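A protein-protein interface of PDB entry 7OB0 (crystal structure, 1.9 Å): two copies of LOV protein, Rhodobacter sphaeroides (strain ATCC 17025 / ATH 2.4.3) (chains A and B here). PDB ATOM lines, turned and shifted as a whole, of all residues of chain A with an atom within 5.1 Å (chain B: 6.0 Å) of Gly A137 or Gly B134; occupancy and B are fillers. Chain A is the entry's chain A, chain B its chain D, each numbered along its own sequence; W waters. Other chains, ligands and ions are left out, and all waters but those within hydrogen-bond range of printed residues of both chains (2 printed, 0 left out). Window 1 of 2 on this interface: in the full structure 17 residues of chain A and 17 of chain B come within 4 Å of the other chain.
Among the printed residues, merely in contact across the chains: Ala A133 with Ala B130, Ala A133 with Ala B133, Ala A133 with Gly B134, Gly A134 with Ala B133, Gly A134 with Gly B137, Gly A137 with Gly B134, Gly A137 with Ala B138, Ala A138 with Gly B137, Ala A138 with Ala B138, Arg A158 with Gly B134, Arg A158 with Ala B138 and Ala A162 with Ala B130.
Of chain B, only Gly B134 (3.3 Å) and Ala B138 (3.6 Å) come within 4 Å of Gly A137.
Of the printed residues of chain A, Gly B134 touches Ala A133 (3.3 Å), Gly A137 (3.3 Å) and Arg A158 (3.6 Å).
Printed residues of chain B within 4 Å of Arg A158: Gly B134 and Ala B138.
Of the printed residues of chain B, Gly A134 touches Ala B133 (3.4 Å) and Gly B137 (3.3 Å).
Of the printed residues of chain A, Ala B130 touches Ala A133 and Ala A162.
Of the printed residues of chain A, Ala B138 touches Gly A137, Ala A138 and Arg A158.
Of the printed residues of chain B, Ala A138 touches Gly B137 and Ala B138.
Ala B132 touches none of the printed residues of chain A.
Leu A139 touches none of the printed residues of chain B.
The nearest residue of chain B that does not touch Gly A137 is Gly B137 (4.2 Å).
The nearest printed residue of chain A that does not touch Ala B133 is Ala A162 (5.6 Å).
Hydrophobic or aromatic side chains of chain B that line the printed part of chain A: Ala B130, Ala B133 and Ala B138.
Among the printed residues, 12 pairs touch across the chains.
Among the printed residues, no Asp or Glu carboxylate lies within 4 Å of a Lys or Arg side-chain nitrogen of the other chain.
Ala B133 touches its own counterpart, Ala A133.
Ala A133 touches Gly B134, and with the chains exchanged Gly A134 touches Ala B133.
Gly A134 touches Gly B137, and with the chains exchanged Gly A137 touches Gly B134.
Ala B138 touches its own counterpart, Ala A138.
Of the 12 pairs that touch across the chains among the printed residues, 8 have their exchanged pair printed and touching as well.
Water W2 bridges the guanidinium group of Arg A158 and a ring nitrogen (ND1) of His B135.
Water W1 lies within hydrogen-bond range of O of Ala B131 and NE of Arg A158.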
ATOM      1  N   ALA A 133      11.224   8.868 -21.153  1.00  0.00           N
ATOM      2  CA  ALA A 133      10.957  10.249 -20.748  1.00  0.00           C
ATOM      3  C   ALA A 133      11.226  10.430 -19.259  1.00  0.00           C
ATOM      4  O   ALA A 133      11.733  11.467 -18.831  1.00  0.00           O
ATOM      5  CB  ALA A 133       9.515  10.628 -21.085  1.00  0.00           C
ATOM      6  N   GLY A 134      10.914   9.414 -18.453  1.00  0.00           N
ATOM      7  CA  GLY A 134      11.245   9.485 -17.039  1.00  0.00           C
ATOM      8  C   GLY A 134      12.739   9.601 -16.803  1.00  0.00           C
ATOM      9  O   GLY A 134      13.192  10.379 -15.959  1.00  0.00           O
ATOM     10  N   HIS A 135      13.520   8.820 -17.536  1.00  0.00           N
ATOM     11  CA  HIS A 135      14.971   8.944 -17.443  1.00  0.00           C
ATOM     12  C   HIS A 135      15.411  10.356 -17.813  1.00  0.00           C
ATOM     13  O   HIS A 135      16.232  10.957 -17.125  1.00  0.00           O
ATOM     14  CB  HIS A 135      15.631   7.921 -18.366  1.00  0.00           C
ATOM     15  CG  HIS A 135      17.120   7.938 -18.307  1.00  0.00           C
ATOM     16  ND1 HIS A 135      17.849   6.943 -17.692  1.00  0.00           N
ATOM     17  CD2 HIS A 135      18.021   8.830 -18.785  1.00  0.00           C
ATOM     18  CE1 HIS A 135      19.138   7.226 -17.791  1.00  0.00           C
ATOM     19  NE2 HIS A 135      19.268   8.369 -18.444  1.00  0.00           N
ATOM     20  N   ALA A 136      14.836  10.911 -18.882  1.00  0.00           N
ATOM     21  CA  ALA A 136      15.214  12.253 -19.316  1.00  0.00           C
ATOM     22  C   ALA A 136      14.931  13.284 -18.232  1.00  0.00           C
ATOM     23  O   ALA A 136      15.689  14.246 -18.065  1.00  0.00           O
ATOM     24  CB  ALA A 136      14.462  12.609 -20.602  1.00  0.00           C
ATOM     25  N   GLY A 137      13.833  13.111 -17.498  1.00  0.00           N
ATOM     26  CA  GLY A 137      13.512  14.050 -16.433  1.00  0.00           C
ATOM     27  C   GLY A 137      14.463  13.945 -15.253  1.00  0.00           C
ATOM     28  O   GLY A 137      14.877  14.961 -14.693  1.00  0.00           O
ATOM     29  N   ALA A 138      14.812  12.709 -14.853  1.00  0.00           N
ATOM     30  CA  ALA A 138      15.812  12.521 -13.801  1.00  0.00           C
ATOM     31  C   ALA A 138      17.163  13.082 -14.225  1.00  0.00           C
ATOM     32  O   ALA A 138      17.858  13.726 -13.432  1.00  0.00           O
ATOM     33  CB  ALA A 138      15.958  11.033 -13.473  1.00  0.00           C
ATOM     34  N   LEU A 139      17.548  12.823 -15.474  1.00  0.00           N
ATOM     35  CA  LEU A 139      18.792  13.356 -16.017  1.00  0.00           C
ATOM     36  C   LEU A 139      18.804  14.885 -15.975  1.00  0.00           C
ATOM     37  O   LEU A 139      19.800  15.503 -15.578  1.00  0.00           O
ATOM     38  CB  LEU A 139      18.967  12.855 -17.453  1.00  0.00           C
ATOM     39  CG  LEU A 139      20.101  13.568 -18.193  1.00  0.00           C
ATOM     40  CD1 LEU A 139      21.460  13.302 -17.528  1.00  0.00           C
ATOM     41  CD2 LEU A 139      20.097  13.200 -19.670  1.00  0.00           C
ATOM     42  N   THR A 140      17.709  15.515 -16.413  1.00  0.00           N
ATOM     43  CA  THR A 140      17.647  16.979 -16.386  1.00  0.00           C
ATOM     44  C   THR A 140      17.893  17.509 -14.976  1.00  0.00           C
ATOM     45  O   THR A 140      18.600  18.512 -14.788  1.00  0.00           O
ATOM     46  CB  THR A 140      16.284  17.450 -16.936  1.00  0.00           C
ATOM     47  OG1 THR A 140      16.132  17.024 -18.298  1.00  0.00           O
ATOM     48  CG2 THR A 140      16.176  18.966 -16.905  1.00  0.00           C
ATOM     49  N   GLY A 141      17.346  16.834 -13.964  1.00  0.00           N
ATOM     50  CA  GLY A 141      17.630  17.224 -12.588  1.00  0.00           C
ATOM     51  C   GLY A 141      19.113  17.181 -12.254  1.00  0.00           C
ATOM     52  O   GLY A 141      19.625  18.055 -11.542  1.00  0.00           O
ATOM     53  N   ARG A 158      13.539  19.842 -19.538  1.00  0.00           N
ATOM     54  CA  ARG A 158      12.949  18.575 -19.137  1.00  0.00           C
ATOM     55  C   ARG A 158      11.887  18.137 -20.136  1.00  0.00           C
ATOM     56  O   ARG A 158      11.870  16.983 -20.576  1.00  0.00           O
ATOM     57  CB  ARG A 158      12.366  18.705 -17.728  1.00  0.00           C
ATOM     58  CG  ARG A 158      11.839  17.408 -17.144  1.00  0.00           C
ATOM     59  CD  ARG A 158      11.536  17.564 -15.658  1.00  0.00           C
ATOM     60  NE  ARG A 158      10.604  18.650 -15.393  1.00  0.00           N
ATOM     61  CZ  ARG A 158      10.878  19.756 -14.714  1.00  0.00           C
ATOM     62  NH1 ARG A 158      12.070  19.972 -14.181  1.00  0.00           N
ATOM     63  NH2 ARG A 158       9.929  20.677 -14.576  1.00  0.00           N
ATOM     64  N   ALA A 162      12.504  14.908 -22.624  1.00  0.00           N
ATOM     65  CA  ALA A 162      11.496  13.847 -22.561  1.00  0.00           C
ATOM     66  C   ALA A 162      10.858  13.611 -23.929  1.00  0.00           C
ATOM     67  O   ALA A 162      10.628  12.456 -24.323  1.00  0.00           O
ATOM     68  CB  ALA A 162      10.436  14.202 -21.519  1.00  0.00           C
ATOM     69  N   GLU B 129       2.114  13.849 -22.594  1.00  0.00           N
ATOM     70  CA  GLU B 129       2.441  12.560 -21.985  1.00  0.00           C
ATOM     71  C   GLU B 129       3.909  12.489 -21.616  1.00  0.00           C
ATOM     72  O   GLU B 129       4.267  12.053 -20.517  1.00  0.00           O
ATOM     73  CB  GLU B 129       2.114  11.416 -22.933  1.00  0.00           C
ATOM     74  CG  GLU B 129       0.679  11.097 -23.050  1.00  0.00           C
ATOM     75  CD  GLU B 129       0.483  10.005 -24.068  1.00  0.00           C
ATOM     76  OE1 GLU B 129       0.944   8.878 -23.801  1.00  0.00           O
ATOM     77  OE2 GLU B 129      -0.115  10.283 -25.123  1.00  0.00           O
ATOM     78  N   ALA B 130       4.782  12.900 -22.537  1.00  0.00           N
ATOM     79  CA  ALA B 130       6.207  12.765 -22.280  1.00  0.00           C
ATOM     80  C   ALA B 130       6.655  13.753 -21.214  1.00  0.00           C
ATOM     81  O   ALA B 130       7.470  13.413 -20.346  1.00  0.00           O
ATOM     82  CB  ALA B 130       6.993  12.949 -23.580  1.00  0.00           C
ATOM     83  N   ALA B 131       6.103  14.972 -21.234  1.00  0.00           N
ATOM     84  CA  ALA B 131       6.508  15.953 -20.238  1.00  0.00           C
ATOM     85  C   ALA B 131       6.059  15.529 -18.845  1.00  0.00           C
ATOM     86  O   ALA B 131       6.785  15.727 -17.864  1.00  0.00           O
ATOM     87  CB  ALA B 131       5.954  17.341 -20.598  1.00  0.00           C
ATOM     88  N   ALA B 132       4.870  14.934 -18.736  1.00  0.00           N
ATOM     89  CA  ALA B 132       4.420  14.453 -17.434  1.00  0.00           C
ATOM     90  C   ALA B 132       5.285  13.296 -16.951  1.00  0.00           C
ATOM     91  O   ALA B 132       5.596  13.203 -15.754  1.00  0.00           O
ATOM     92  CB  ALA B 132       2.954  14.027 -17.498  1.00  0.00           C
ATOM     93  N   ALA B 133       5.657  12.391 -17.861  1.00  0.00           N
ATOM     94  CA  ALA B 133       6.593  11.328 -17.502  1.00  0.00           C
ATOM     95  C   ALA B 133       7.944  11.915 -17.115  1.00  0.00           C
ATOM     96  O   ALA B 133       8.583  11.458 -16.153  1.00  0.00           O
ATOM     97  CB  ALA B 133       6.747  10.334 -18.656  1.00  0.00           C
ATOM     98  N   GLY B 134       8.387  12.944 -17.843  1.00  0.00           N
ATOM     99  CA  GLY B 134       9.599  13.641 -17.446  1.00  0.00           C
ATOM    100  C   GLY B 134       9.506  14.199 -16.039  1.00  0.00           C
ATOM    101  O   GLY B 134      10.455  14.106 -15.254  1.00  0.00           O
ATOM    102  N   HIS B 135       8.358  14.775 -15.695  1.00  0.00           N
ATOM    103  CA  HIS B 135       8.190  15.302 -14.350  1.00  0.00           C
ATOM    104  C   HIS B 135       8.234  14.173 -13.331  1.00  0.00           C
ATOM    105  O   HIS B 135       8.870  14.306 -12.283  1.00  0.00           O
ATOM    106  CB  HIS B 135       6.870  16.083 -14.258  1.00  0.00           C
ATOM    107  CG  HIS B 135       6.604  16.669 -12.908  1.00  0.00           C
ATOM    108  ND1 HIS B 135       6.638  18.029 -12.674  1.00  0.00           N
ATOM    109  CD2 HIS B 135       6.272  16.092 -11.728  1.00  0.00           C
ATOM    110  CE1 HIS B 135       6.364  18.261 -11.403  1.00  0.00           C
ATOM    111  NE2 HIS B 135       6.127  17.103 -10.808  1.00  0.00           N
ATOM    112  N   ALA B 136       7.575  13.053 -13.630  1.00  0.00           N
ATOM    113  CA  ALA B 136       7.610  11.905 -12.722  1.00  0.00           C
ATOM    114  C   ALA B 136       9.038  11.452 -12.453  1.00  0.00           C
ATOM    115  O   ALA B 136       9.370  11.080 -11.325  1.00  0.00           O
ATOM    116  CB  ALA B 136       6.787  10.751 -13.295  1.00  0.00           C
ATOM    117  N   GLY B 137       9.893  11.461 -13.480  1.00  0.00           N
ATOM    118  CA  GLY B 137      11.273  11.027 -13.292  1.00  0.00           C
ATOM    119  C   GLY B 137      12.084  11.991 -12.444  1.00  0.00           C
ATOM    120  O   GLY B 137      12.872  11.572 -11.590  1.00  0.00           O
ATOM    121  N   ALA B 138      11.911  13.297 -12.667  1.00  0.00           N
ATOM    122  CA  ALA B 138      12.557  14.275 -11.798  1.00  0.00           C
ATOM    123  C   ALA B 138      12.064  14.117 -10.363  1.00  0.00           C
ATOM    124  O   ALA B 138      12.861  14.087  -9.418  1.00  0.00           O
ATOM    125  CB  ALA B 138      12.297  15.690 -12.330  1.00  0.00           C
ATOM    126  N   LEU B 139      10.744  13.979 -10.189  1.00  0.00           N
ATOM    127  CA  LEU B 139      10.166  13.783  -8.865  1.00  0.00           C
ATOM    128  C   LEU B 139      10.745  12.556  -8.176  1.00  0.00           C
ATOM    129  O   LEU B 139      11.073  12.602  -6.987  1.00  0.00           O
ATOM    130  CB  LEU B 139       8.641  13.652  -8.980  1.00  0.00           C
ATOM    131  CG  LEU B 139       7.884  13.219  -7.726  1.00  0.00           C
ATOM    132  CD1 LEU B 139       8.070  14.200  -6.577  1.00  0.00           C
ATOM    133  CD2 LEU B 139       6.417  13.034  -8.070  1.00  0.00           C
ATOM    134  N   ALA B 162       6.285   7.213 -14.024  1.00  0.00           N
ATOM    135  CA  ALA B 162       6.217   7.784 -15.365  1.00  0.00           C
ATOM    136  C   ALA B 162       5.081   7.166 -16.178  1.00  0.00           C
ATOM    137  O   ALA B 162       4.365   7.885 -16.887  1.00  0.00           O
ATOM    138  CB  ALA B 162       7.554   7.606 -16.094  1.00  0.00           C
HETATM  139  O   HOH W   1       8.169  17.999 -17.304  1.00  0.00           O
HETATM  140  O   HOH W   2       7.400  19.814 -14.583  1.00  0.00           O
